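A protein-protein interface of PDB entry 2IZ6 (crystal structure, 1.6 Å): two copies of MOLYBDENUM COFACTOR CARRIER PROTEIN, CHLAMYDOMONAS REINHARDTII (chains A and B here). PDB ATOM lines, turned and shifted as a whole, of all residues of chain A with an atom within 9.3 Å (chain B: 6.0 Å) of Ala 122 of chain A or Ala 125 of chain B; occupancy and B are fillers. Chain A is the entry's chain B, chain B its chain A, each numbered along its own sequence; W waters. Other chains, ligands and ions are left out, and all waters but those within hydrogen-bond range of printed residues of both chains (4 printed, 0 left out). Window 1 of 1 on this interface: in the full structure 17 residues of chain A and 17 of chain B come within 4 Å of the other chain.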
ATOM      1  N   MET A  19     -27.390  12.672  -1.573  1.00  0.00           N
ATOM      2  CA  MET A  19     -25.953  12.697  -1.495  1.00  0.00           C
ATOM      3  C   MET A  19     -25.379  11.326  -1.713  1.00  0.00           C
ATOM      4  O   MET A  19     -25.994  10.341  -1.473  1.00  0.00           O
ATOM      5  CB  MET A  19     -25.481  13.215  -0.118  1.00  0.00           C
ATOM      6  CG  MET A  19     -23.944  13.334   0.071  1.00  0.00           C
ATOM      7  SD  MET A  19     -23.059  14.373  -1.134  1.00  0.00           S
ATOM      8  CE  MET A  19     -24.100  15.811  -0.888  1.00  0.00           C
ATOM      9  N   ALA A  99     -13.857  21.692  -1.079  1.00  0.00           N
ATOM     10  CA  ALA A  99     -13.303  20.972   0.086  1.00  0.00           C
ATOM     11  C   ALA A  99     -14.428  20.253   0.832  1.00  0.00           C
ATOM     12  O   ALA A  99     -14.198  19.234   1.552  1.00  0.00           O
ATOM     13  CB  ALA A  99     -12.564  21.926   1.013  1.00  0.00           C
ATOM     14  N   ARG A 100     -15.647  20.743   0.620  1.00  0.00           N
ATOM     15  CA  ARG A 100     -16.859  20.139   1.136  1.00  0.00           C
ATOM     16  C   ARG A 100     -17.840  19.909   0.002  1.00  0.00           C
ATOM     17  O   ARG A 100     -17.949  20.758  -0.889  1.00  0.00           O
ATOM     18  CB  ARG A 100     -17.467  21.080   2.173  1.00  0.00           C
ATOM     19  CG  ARG A 100     -18.707  20.598   2.755  1.00  0.00           C
ATOM     20  CD  ARG A 100     -19.293  21.599   3.718  1.00  0.00           C
ATOM     21  NE  ARG A 100     -20.649  21.273   3.957  1.00  0.00           N
ATOM     22  CZ  ARG A 100     -21.486  22.016   4.669  1.00  0.00           C
ATOM     23  NH1 ARG A 100     -21.095  23.166   5.214  1.00  0.00           N
ATOM     24  NH2 ARG A 100     -22.714  21.609   4.817  1.00  0.00           N
ATOM     25  N   ASP A 101     -18.548  18.784   0.000  1.00  0.00           N
ATOM     26  CA  ASP A 101     -19.554  18.501  -1.040  1.00  0.00           C
ATOM     27  C   ASP A 101     -20.891  19.173  -0.647  1.00  0.00           C
ATOM     28  O   ASP A 101     -21.907  18.510  -0.374  1.00  0.00           O
ATOM     29  CB  ASP A 101     -19.766  16.992  -1.227  1.00  0.00           C
ATOM     30  CG  ASP A 101     -18.579  16.279  -1.839  1.00  0.00           C
ATOM     31  OD1 ASP A 101     -17.843  16.880  -2.665  1.00  0.00           O
ATOM     32  OD2 ASP A 101     -18.440  15.064  -1.492  1.00  0.00           O
ATOM     33  N   ASN A 102     -20.866  20.500  -0.631  1.00  0.00           N
ATOM     34  CA  ASN A 102     -21.988  21.297  -0.137  1.00  0.00           C
ATOM     35  C   ASN A 102     -23.096  21.305  -1.187  1.00  0.00           C
ATOM     36  O   ASN A 102     -22.861  21.742  -2.335  1.00  0.00           O
ATOM     37  CB  ASN A 102     -21.459  22.714   0.117  1.00  0.00           C
ATOM     38  CG  ASN A 102     -22.353  23.556   1.006  1.00  0.00           C
ATOM     39  OD1 ASN A 102     -23.571  23.396   0.989  1.00  0.00           O
ATOM     40  ND2 ASN A 102     -21.730  24.477   1.807  1.00  0.00           N
ATOM     41  N   ALA A 105     -27.682  21.483   1.598  1.00  0.00           N
ATOM     42  CA  ALA A 105     -28.653  20.465   2.099  1.00  0.00           C
ATOM     43  C   ALA A 105     -29.668  20.862   3.166  1.00  0.00           C
ATOM     44  O   ALA A 105     -30.675  20.155   3.320  1.00  0.00           O
ATOM     45  CB  ALA A 105     -27.841  19.258   2.658  1.00  0.00           C
ATOM     46  N   LEU A 111     -32.900  14.331   3.733  1.00  0.00           N
ATOM     47  CA  LEU A 111     -31.649  14.035   2.992  1.00  0.00           C
ATOM     48  C   LEU A 111     -31.551  12.498   2.856  1.00  0.00           C
ATOM     49  O   LEU A 111     -31.720  11.811   3.872  1.00  0.00           O
ATOM     50  CB  LEU A 111     -30.424  14.570   3.753  1.00  0.00           C
ATOM     51  CG  LEU A 111     -29.061  14.319   3.110  1.00  0.00           C
ATOM     52  CD1 LEU A 111     -28.961  15.005   1.736  1.00  0.00           C
ATOM     53  CD2 LEU A 111     -27.909  14.800   3.959  1.00  0.00           C
ATOM     54  N   ALA A 113     -28.932   9.522   1.608  1.00  0.00           N
ATOM     55  CA  ALA A 113     -27.567   9.153   1.128  1.00  0.00           C
ATOM     56  C   ALA A 113     -27.679   7.807   0.463  1.00  0.00           C
ATOM     57  O   ALA A 113     -28.272   6.882   1.000  1.00  0.00           O
ATOM     58  CB  ALA A 113     -26.596   9.084   2.262  1.00  0.00           C
ATOM     59  N   MET A 116     -21.684   5.594   0.316  1.00  0.00           N
ATOM     60  CA  MET A 116     -20.942   6.258   1.416  1.00  0.00           C
ATOM     61  C   MET A 116     -19.532   6.537   1.003  1.00  0.00           C
ATOM     62  O   MET A 116     -18.941   5.890   0.125  1.00  0.00           O
ATOM     63  CB  MET A 116     -20.981   5.406   2.670  1.00  0.00           C
ATOM     64  CG  MET A 116     -20.467   6.091   3.967  1.00  0.00           C
ATOM     65  SD  MET A 116     -21.152   7.670   4.318  1.00  0.00           S
ATOM     66  CE  MET A 116     -22.921   7.382   4.376  1.00  0.00           C
ATOM     67  N   GLY A 117     -18.977   7.607   1.556  1.00  0.00           N
ATOM     68  CA  GLY A 117     -17.628   8.077   1.280  1.00  0.00           C
ATOM     69  C   GLY A 117     -17.398   9.296   2.226  1.00  0.00           C
ATOM     70  O   GLY A 117     -18.348   9.764   2.900  1.00  0.00           O
ATOM     71  N   PRO A 118     -16.157   9.780   2.338  1.00  0.00           N
ATOM     72  CA  PRO A 118     -15.879  10.920   3.261  1.00  0.00           C
ATOM     73  C   PRO A 118     -16.800  12.111   3.051  1.00  0.00           C
ATOM     74  O   PRO A 118     -17.412  12.634   4.028  1.00  0.00           O
ATOM     75  CB  PRO A 118     -14.406  11.243   2.980  1.00  0.00           C
ATOM     76  CG  PRO A 118     -13.864   9.947   2.701  1.00  0.00           C
ATOM     77  CD  PRO A 118     -14.915   9.310   1.747  1.00  0.00           C
ATOM     78  N   GLY A 119     -16.998  12.593   1.820  1.00  0.00           N
ATOM     79  CA  GLY A 119     -17.841  13.750   1.599  1.00  0.00           C
ATOM     80  C   GLY A 119     -19.271  13.485   1.962  1.00  0.00           C
ATOM     81  O   GLY A 119     -19.941  14.312   2.579  1.00  0.00           O
ATOM     82  N   THR A 120     -19.780  12.296   1.640  1.00  0.00           N
ATOM     83  CA  THR A 120     -21.146  11.932   1.996  1.00  0.00           C
ATOM     84  C   THR A 120     -21.320  11.874   3.552  1.00  0.00           C
ATOM     85  O   THR A 120     -22.264  12.368   4.118  1.00  0.00           O
ATOM     86  CB  THR A 120     -21.568  10.567   1.347  1.00  0.00           C
ATOM     87  OG1 THR A 120     -21.549  10.734  -0.085  1.00  0.00           O
ATOM     88  CG2 THR A 120     -22.977  10.152   1.844  1.00  0.00           C
ATOM     89  N   ALA A 121     -20.358  11.262   4.202  1.00  0.00           N
ATOM     90  CA  ALA A 121     -20.350  11.164   5.668  1.00  0.00           C
ATOM     91  C   ALA A 121     -20.466  12.529   6.347  1.00  0.00           C
ATOM     92  O   ALA A 121     -21.183  12.692   7.323  1.00  0.00           O
ATOM     93  CB  ALA A 121     -19.060  10.436   6.123  1.00  0.00           C
ATOM     94  N   ALA A 122     -19.755  13.515   5.794  1.00  0.00           N
ATOM     95  CA  ALA A 122     -19.724  14.861   6.361  1.00  0.00           C
ATOM     96  C   ALA A 122     -21.095  15.486   6.198  1.00  0.00           C
ATOM     97  O   ALA A 122     -21.642  16.072   7.100  1.00  0.00           O
ATOM     98  CB  ALA A 122     -18.645  15.756   5.610  1.00  0.00           C
ATOM     99  N   GLU A 123     -21.730  15.338   5.041  1.00  0.00           N
ATOM    100  CA  GLU A 123     -23.036  15.893   4.820  1.00  0.00           C
ATOM    101  C   GLU A 123     -24.121  15.235   5.659  1.00  0.00           C
ATOM    102  O   GLU A 123     -24.996  15.928   6.177  1.00  0.00           O
ATOM    103  CB  GLU A 123     -23.437  15.904   3.346  1.00  0.00           C
ATOM    104  CG  GLU A 123     -22.646  16.823   2.515  1.00  0.00           C
ATOM    105  CD  GLU A 123     -22.543  18.275   3.060  1.00  0.00           C
ATOM    106  OE1 GLU A 123     -23.536  18.927   3.453  1.00  0.00           O
ATOM    107  OE2 GLU A 123     -21.406  18.700   3.179  1.00  0.00           O
ATOM    108  N   VAL A 124     -24.039  13.918   5.844  1.00  0.00           N
ATOM    109  CA  VAL A 124     -24.968  13.217   6.707  1.00  0.00           C
ATOM    110  C   VAL A 124     -24.747  13.714   8.137  1.00  0.00           C
ATOM    111  O   VAL A 124     -25.686  13.998   8.853  1.00  0.00           O
ATOM    112  CB  VAL A 124     -24.798  11.693   6.605  1.00  0.00           C
ATOM    113  CG1 VAL A 124     -25.637  10.982   7.684  1.00  0.00           C
ATOM    114  CG2 VAL A 124     -25.133  11.210   5.198  1.00  0.00           C
ATOM    115  N   ALA A 125     -23.507  13.765   8.578  1.00  0.00           N
ATOM    116  CA  ALA A 125     -23.276  14.237   9.991  1.00  0.00           C
ATOM    117  C   ALA A 125     -23.792  15.648  10.218  1.00  0.00           C
ATOM    118  O   ALA A 125     -24.391  15.969  11.234  1.00  0.00           O
ATOM    119  CB  ALA A 125     -21.817  14.159  10.361  1.00  0.00           C
ATOM    120  N   LEU A 126     -23.589  16.536   9.246  1.00  0.00           N
ATOM    121  CA  LEU A 126     -24.061  17.950   9.368  1.00  0.00           C
ATOM    122  C   LEU A 126     -25.584  18.024   9.349  1.00  0.00           C
ATOM    123  O   LEU A 126     -26.192  18.879  10.015  1.00  0.00           O
ATOM    124  CB  LEU A 126     -23.387  18.876   8.326  1.00  0.00           C
ATOM    125  CG  LEU A 126     -21.883  19.041   8.520  1.00  0.00           C
ATOM    126  CD1 LEU A 126     -21.252  19.866   7.349  1.00  0.00           C
ATOM    127  CD2 LEU A 126     -21.562  19.664   9.891  1.00  0.00           C
ATOM    128  N   ALA A 127     -26.224  17.170   8.572  1.00  0.00           N
ATOM    129  CA  ALA A 127     -27.703  17.122   8.597  1.00  0.00           C
ATOM    130  C   ALA A 127     -28.176  16.750   9.996  1.00  0.00           C
ATOM    131  O   ALA A 127     -29.077  17.380  10.552  1.00  0.00           O
ATOM    132  CB  ALA A 127     -28.213  16.133   7.562  1.00  0.00           C
ATOM    133  N   LEU A 128     -27.558  15.742  10.610  1.00  0.00           N
ATOM    134  CA  LEU A 128     -27.917  15.309  11.960  1.00  0.00           C
ATOM    135  C   LEU A 128     -27.630  16.424  12.984  1.00  0.00           C
ATOM    136  O   LEU A 128     -28.397  16.637  13.930  1.00  0.00           O
ATOM    137  CB  LEU A 128     -27.150  14.062  12.347  1.00  0.00           C
ATOM    138  CG  LEU A 128     -27.481  12.830  11.492  1.00  0.00           C
ATOM    139  CD1 LEU A 128     -26.649  11.624  11.928  1.00  0.00           C
ATOM    140  CD2 LEU A 128     -28.961  12.507  11.615  1.00  0.00           C
ATOM    141  N   LYS A 129     -26.514  17.131  12.816  1.00  0.00           N
ATOM    142  CA  LYS A 129     -26.222  18.315  13.627  1.00  0.00           C
ATOM    143  C   LYS A 129     -27.364  19.375  13.635  1.00  0.00           C
ATOM    144  O   LYS A 129     -27.676  19.976  14.684  1.00  0.00           O
ATOM    145  CB  LYS A 129     -24.882  18.931  13.197  1.00  0.00           C
ATOM    146  CG  LYS A 129     -24.484  20.067  14.083  1.00  0.00           C
ATOM    147  CD  LYS A 129     -23.066  20.527  13.800  1.00  0.00           C
ATOM    148  CE  LYS A 129     -22.728  21.905  14.377  1.00  0.00           C
ATOM    149  NZ  LYS A 129     -22.955  22.019  15.808  1.00  0.00           N
ATOM    150  N   ALA A 130     -27.970  19.550  12.446  1.00  0.00           N
ATOM    151  CA  ALA A 130     -29.042  20.500  12.243  1.00  0.00           C
ATOM    152  C   ALA A 130     -30.403  19.880  12.601  1.00  0.00           C
ATOM    153  O   ALA A 130     -31.467  20.530  12.440  1.00  0.00           O
ATOM    154  CB  ALA A 130     -28.989  20.915  10.855  1.00  0.00           C
ATOM    155  N   VAL A 134     -32.272  11.818   8.108  1.00  0.00           N
ATOM    156  CA  VAL A 134     -31.460  11.231   7.029  1.00  0.00           C
ATOM    157  C   VAL A 134     -31.890   9.789   6.784  1.00  0.00           C
ATOM    158  O   VAL A 134     -32.177   9.064   7.703  1.00  0.00           O
ATOM    159  CB  VAL A 134     -29.936  11.238   7.332  1.00  0.00           C
ATOM    160  CG1 VAL A 134     -29.178  10.614   6.159  1.00  0.00           C
ATOM    161  CG2 VAL A 134     -29.466  12.651   7.598  1.00  0.00           C
ATOM    162  N   PHE A 146     -22.804   3.432  12.781  1.00  0.00           N
ATOM    163  CA  PHE A 146     -22.178   4.687  13.231  1.00  0.00           C
ATOM    164  C   PHE A 146     -23.166   5.861  13.264  1.00  0.00           C
ATOM    165  O   PHE A 146     -23.313   6.529  14.287  1.00  0.00           O
ATOM    166  CB  PHE A 146     -20.992   5.085  12.376  1.00  0.00           C
ATOM    167  CG  PHE A 146     -20.466   6.442  12.768  1.00  0.00           C
ATOM    168  CD1 PHE A 146     -19.998   6.654  14.069  1.00  0.00           C
ATOM    169  CD2 PHE A 146     -20.476   7.515  11.857  1.00  0.00           C
ATOM    170  CE1 PHE A 146     -19.533   7.924  14.450  1.00  0.00           C
ATOM    171  CE2 PHE A 146     -19.964   8.762  12.241  1.00  0.00           C
ATOM    172  CZ  PHE A 146     -19.534   8.957  13.557  1.00  0.00           C
ATOM    173  N   PHE A 147     -23.904   6.092  12.173  1.00  0.00           N
ATOM    174  CA  PHE A 147     -24.875   7.173  12.206  1.00  0.00           C
ATOM    175  C   PHE A 147     -25.966   6.985  13.191  1.00  0.00           C
ATOM    176  O   PHE A 147     -26.327   7.896  13.854  1.00  0.00           O
ATOM    177  CB  PHE A 147     -25.364   7.504  10.800  1.00  0.00           C
ATOM    178  CG  PHE A 147     -24.287   8.114   9.974  1.00  0.00           C
ATOM    179  CD1 PHE A 147     -23.771   9.340  10.382  1.00  0.00           C
ATOM    180  CD2 PHE A 147     -23.679   7.458   8.925  1.00  0.00           C
ATOM    181  CE1 PHE A 147     -22.786   9.932   9.732  1.00  0.00           C
ATOM    182  CE2 PHE A 147     -22.636   8.126   8.216  1.00  0.00           C
ATOM    183  CZ  PHE A 147     -22.199   9.364   8.690  1.00  0.00           C
ATOM    184  N   LEU A 150     -24.938   8.233  16.461  1.00  0.00           N
ATOM    185  CA  LEU A 150     -24.913   9.705  16.596  1.00  0.00           C
ATOM    186  C   LEU A 150     -26.264  10.235  16.970  1.00  0.00           C
ATOM    187  O   LEU A 150     -26.337  11.053  17.852  1.00  0.00           O
ATOM    188  CB  LEU A 150     -24.456  10.414  15.328  1.00  0.00           C
ATOM    189  CG  LEU A 150     -22.993  10.226  14.888  1.00  0.00           C
ATOM    190  CD1 LEU A 150     -22.767  11.034  13.639  1.00  0.00           C
ATOM    191  CD2 LEU A 150     -21.982  10.590  15.960  1.00  0.00           C
ATOM    192  N   THR B 120     -18.142  16.872  15.237  1.00  0.00           N
ATOM    193  CA  THR B 120     -16.853  16.244  15.224  1.00  0.00           C
ATOM    194  C   THR B 120     -16.742  15.283  14.044  1.00  0.00           C
ATOM    195  O   THR B 120     -15.779  15.285  13.362  1.00  0.00           O
ATOM    196  CB  THR B 120     -16.533  15.616  16.571  1.00  0.00           C
ATOM    197  OG1 THR B 120     -16.446  16.743  17.434  1.00  0.00           O
ATOM    198  CG2 THR B 120     -15.171  14.912  16.515  1.00  0.00           C
ATOM    199  N   ALA B 121     -17.755  14.481  13.876  1.00  0.00           N
ATOM    200  CA  ALA B 121     -17.777  13.494  12.787  1.00  0.00           C
ATOM    201  C   ALA B 121     -17.645  14.162  11.430  1.00  0.00           C
ATOM    202  O   ALA B 121     -16.955  13.636  10.537  1.00  0.00           O
ATOM    203  CB  ALA B 121     -18.999  12.697  12.876  1.00  0.00           C
ATOM    204  N   ALA B 122     -18.291  15.300  11.256  1.00  0.00           N
ATOM    205  CA  ALA B 122     -18.177  15.993   9.972  1.00  0.00           C
ATOM    206  C   ALA B 122     -16.766  16.457   9.737  1.00  0.00           C
ATOM    207  O   ALA B 122     -16.172  16.360   8.676  1.00  0.00           O
ATOM    208  CB  ALA B 122     -19.125  17.163   9.877  1.00  0.00           C
ATOM    209  N   GLU B 123     -16.158  17.030  10.738  1.00  0.00           N
ATOM    210  CA  GLU B 123     -14.817  17.524  10.577  1.00  0.00           C
ATOM    211  C   GLU B 123     -13.784  16.428  10.326  1.00  0.00           C
ATOM    212  O   GLU B 123     -12.814  16.605   9.564  1.00  0.00           O
ATOM    213  CB  GLU B 123     -14.391  18.424  11.756  1.00  0.00           C
ATOM    214  CG  GLU B 123     -15.110  19.723  11.884  1.00  0.00           C
ATOM    215  CD  GLU B 123     -15.252  20.559  10.580  1.00  0.00           C
ATOM    216  OE1 GLU B 123     -16.394  21.019  10.363  1.00  0.00           O
ATOM    217  OE2 GLU B 123     -14.267  20.721   9.824  1.00  0.00           O
ATOM    218  N   VAL B 124     -13.950  15.304  10.986  1.00  0.00           N
ATOM    219  CA  VAL B 124     -13.060  14.160  10.781  1.00  0.00           C
ATOM    220  C   VAL B 124     -13.215  13.677   9.297  1.00  0.00           C
ATOM    221  O   VAL B 124     -12.269  13.424   8.543  1.00  0.00           O
ATOM    222  CB  VAL B 124     -13.344  13.000  11.739  1.00  0.00           C
ATOM    223  CG1 VAL B 124     -12.643  11.735  11.314  1.00  0.00           C
ATOM    224  CG2 VAL B 124     -12.957  13.431  13.132  1.00  0.00           C
ATOM    225  N   ALA B 125     -14.476  13.559   8.865  1.00  0.00           N
ATOM    226  CA  ALA B 125     -14.760  13.104   7.504  1.00  0.00           C
ATOM    227  C   ALA B 125     -14.203  14.067   6.491  1.00  0.00           C
ATOM    228  O   ALA B 125     -13.578  13.642   5.467  1.00  0.00           O
ATOM    229  CB  ALA B 125     -16.209  12.956   7.305  1.00  0.00           C
ATOM    230  N   LEU B 126     -14.306  15.383   6.749  1.00  0.00           N
ATOM    231  CA  LEU B 126     -13.722  16.374   5.821  1.00  0.00           C
ATOM    232  C   LEU B 126     -12.176  16.331   5.827  1.00  0.00           C
ATOM    233  O   LEU B 126     -11.542  16.652   4.788  1.00  0.00           O
ATOM    234  CB  LEU B 126     -14.290  17.751   6.055  1.00  0.00           C
ATOM    235  CG  LEU B 126     -15.768  17.848   5.708  1.00  0.00           C
ATOM    236  CD1 LEU B 126     -16.437  19.202   6.038  1.00  0.00           C
ATOM    237  CD2 LEU B 126     -16.011  17.551   4.233  1.00  0.00           C
ATOM    238  N   ALA B 127     -11.540  16.076   6.931  1.00  0.00           N
ATOM    239  CA  ALA B 127     -10.099  15.880   7.032  1.00  0.00           C
ATOM    240  C   ALA B 127      -9.713  14.715   6.170  1.00  0.00           C
ATOM    241  O   ALA B 127      -8.772  14.795   5.418  1.00  0.00           O
ATOM    242  CB  ALA B 127      -9.656  15.652   8.459  1.00  0.00           C
ATOM    243  N   LEU B 128     -10.442  13.605   6.243  1.00  0.00           N
ATOM    244  CA  LEU B 128     -10.140  12.457   5.385  1.00  0.00           C
ATOM    245  C   LEU B 128     -10.374  12.746   3.961  1.00  0.00           C
ATOM    246  O   LEU B 128      -9.583  12.291   3.131  1.00  0.00           O
ATOM    247  CB  LEU B 128     -10.892  11.199   5.787  1.00  0.00           C
ATOM    248  CG  LEU B 128     -10.642  10.761   7.245  1.00  0.00           C
ATOM    249  CD1 LEU B 128     -11.568   9.624   7.635  1.00  0.00           C
ATOM    250  CD2 LEU B 128      -9.176  10.288   7.445  1.00  0.00           C
ATOM    251  N   LYS B 129     -11.427  13.516   3.635  1.00  0.00           N
ATOM    252  CA  LYS B 129     -11.617  13.921   2.238  1.00  0.00           C
ATOM    253  C   LYS B 129     -10.410  14.694   1.687  1.00  0.00           C
ATOM    254  O   LYS B 129     -10.004  14.517   0.530  1.00  0.00           O
ATOM    255  CB  LYS B 129     -12.915  14.710   2.113  1.00  0.00           C
ATOM    256  CG  LYS B 129     -13.259  15.184   0.724  1.00  0.00           C
ATOM    257  CD  LYS B 129     -14.700  15.813   0.686  1.00  0.00           C
ATOM    258  CE  LYS B 129     -14.980  16.700  -0.561  1.00  0.00           C
ATOM    259  NZ  LYS B 129     -14.514  16.158  -1.859  1.00  0.00           N
ATOM    260  N   ALA B 130      -9.809  15.516   2.557  1.00  0.00           N
ATOM    261  CA  ALA B 130      -8.612  16.292   2.206  1.00  0.00           C
ATOM    262  C   ALA B 130      -7.326  15.462   2.261  1.00  0.00           C
ATOM    263  O   ALA B 130      -6.231  16.039   2.058  1.00  0.00           O
ATOM    264  CB  ALA B 130      -8.484  17.454   3.146  1.00  0.00           C
ATOM    265  N   PHE B 147     -14.604   5.106  10.605  1.00  0.00           N
ATOM    266  CA  PHE B 147     -13.621   5.998  10.006  1.00  0.00           C
ATOM    267  C   PHE B 147     -12.522   5.178   9.432  1.00  0.00           C
ATOM    268  O   PHE B 147     -11.978   5.468   8.370  1.00  0.00           O
ATOM    269  CB  PHE B 147     -13.135   7.100  11.028  1.00  0.00           C
ATOM    270  CG  PHE B 147     -14.178   8.138  11.278  1.00  0.00           C
ATOM    271  CD1 PHE B 147     -14.786   8.263  12.463  1.00  0.00           C
ATOM    272  CD2 PHE B 147     -14.612   8.937  10.232  1.00  0.00           C
ATOM    273  CE1 PHE B 147     -15.841   9.195  12.644  1.00  0.00           C
ATOM    274  CE2 PHE B 147     -15.645   9.887  10.428  1.00  0.00           C
ATOM    275  CZ  PHE B 147     -16.238   9.973  11.587  1.00  0.00           C
ATOM    276  N   LEU B 150     -13.489   4.241   6.033  1.00  0.00           N
ATOM    277  CA  LEU B 150     -13.364   5.356   5.064  1.00  0.00           C
ATOM    278  C   LEU B 150     -11.985   5.485   4.497  1.00  0.00           C
ATOM    279  O   LEU B 150     -11.820   5.757   3.304  1.00  0.00           O
ATOM    280  CB  LEU B 150     -13.775   6.730   5.624  1.00  0.00           C
ATOM    281  CG  LEU B 150     -15.236   6.932   5.985  1.00  0.00           C
ATOM    282  CD1 LEU B 150     -15.461   8.332   6.420  1.00  0.00           C
ATOM    283  CD2 LEU B 150     -16.193   6.580   4.825  1.00  0.00           C
HETATM  284  O   HOH W   1     -16.198  13.749  -2.382  1.00  0.00           O
HETATM  285  O   HOH W   2     -12.005  18.505   2.878  1.00  0.00           O
HETATM  286  O   HOH W   3     -19.097  11.440   9.597  1.00  0.00           O
HETATM  287  O   HOH W   4     -15.686  18.268  -3.682  1.00  0.00           O
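Ala 121 of chain A touches Ala 125 of chain B, but with the chains exchanged Ala 125 of chain A does not touch Ala 121 of chain B (4.1 Å).
Ala 122 of chain A touches its own counterpart, Ala 122 of chain B.
Ala 122 of chain A touches Ala 125 of chain B, and with the chains exchanged Ala 125 of chain A touches Ala 122 of chain B.
Ala 122 of chain A touches Leu 126 of chain B, and with the chains exchanged Leu 126 of chain A touches Ala 122 of chain B.
13 positions are printed for both chains.
Water W2 lies within hydrogen-bond range of O of Ala 99 of chain A (2.7 Å) and O of Leu 126 of chain B (2.7 Å).
Water W1 lies within hydrogen-bond range of OD2 of Asp 101 of chain A (2.7 Å) and NZ of Lys 129 of chain B (3.0 Å).
Water W4 bridges the side-chain carboxylate of Asp 101 of chain A (2.8 Å) and the side-chain amino group of Lys 129 of chain B (3.0 Å).
Water W3 bridges the backbone carbonyl oxygen of Ala 121 of chain B and the backbone carbonyl oxygen of Ala 121 of chain A.
Ala 122 of chain A touches three residues of chain B.
Of the printed residues of chain A, Ala 125 of chain B touches Pro 118 (3.5 Å), Ala 121 (3.98 Å) and Ala 122 (3.9 Å).
No residue of chain A comes within 4 Å of Val 124 of chain B.
Leu 126 of chain B touches just these residues of chain A: Ala 99 (3.6 Å) and Ala 122 (3.5 Å).
Of the printed residues of chain B, Ala 121 of chain A touches Ala 125.
Printed residues of chain B within 4 Å of Pro 118 of chain A: Ala 125 and Lys 129.
Glu 123 of chain A touches none of the printed residues of chain B.
Lys 129 of chain A touches none of the printed residues of chain B.
The nearest residue of chain B that does not touch Ala 122 of chain A is Ala 121 of chain B (5.2 Å).
The nearest printed residue of chain A that does not touch Ala 125 of chain B is Gly 119 of chain A (5.1 Å).
Of the 27 printed residues of chain A, 10 touch a printed residue of chain B.
Along chain A the printed residues that touch a printed residue of chain B span positions 99 to 146.
Of the 13 printed residues of chain B, 7 touch a printed residue of chain A.
Hydrophobic or aromatic side chains of chain B within 4 Å of the printed part of chain A: Ala 121, Ala 122, Ala 125, Leu 126, Phe 147 and Leu 150.
Along chain B the printed residues that touch a printed residue of chain A span positions 121 to 150.
Among the printed residues, 15 pairs touch across the chains.
Among the printed residues, Asp or Glu carboxylates within 4 Å of a Lys or Arg side-chain nitrogen of the other chain: Asp 101 of chain A with Lys 129 of chain B (3.5 Å).
O of Ala 99 of chain A touches CE of Lys 129 of chain B, 3.4 Å away.
Gly 117 of chain A touches Leu 150 of chain B (C to CD2, 3.9 Å).
Ala 125 of chain B touches Pro 118 of chain A (CB to O, 3.5 Å).
Lys 129 of chain B touches Gly 119 of chain A.
Ala 125 of chain B touches Ala 121 of chain A (CB to CB, 3.98 Å).
Ala 122 of chain A touches Ala 122 of chain B (O to CB, 3.9 Å).
Ala 122 of chain B touches Ala 125 of chain A (N to CB, 3.8 Å).
Leu 126 of chain A touches Ala 122 of chain B.
Phe 146 of chain A touches Ala 121 of chain B (CZ to CB, 3.8 Å).
Phe 146 of chain A touches Phe 147 of chain B.
NZ of Lys 129 of chain B lies within salt-bridge range of OD1 of Asp 101 of chain A (3.5 Å).
SD of Met 116 of chain A lies within hydrogen-bond range of N of Ala 121 of chain A (3.7 Å).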
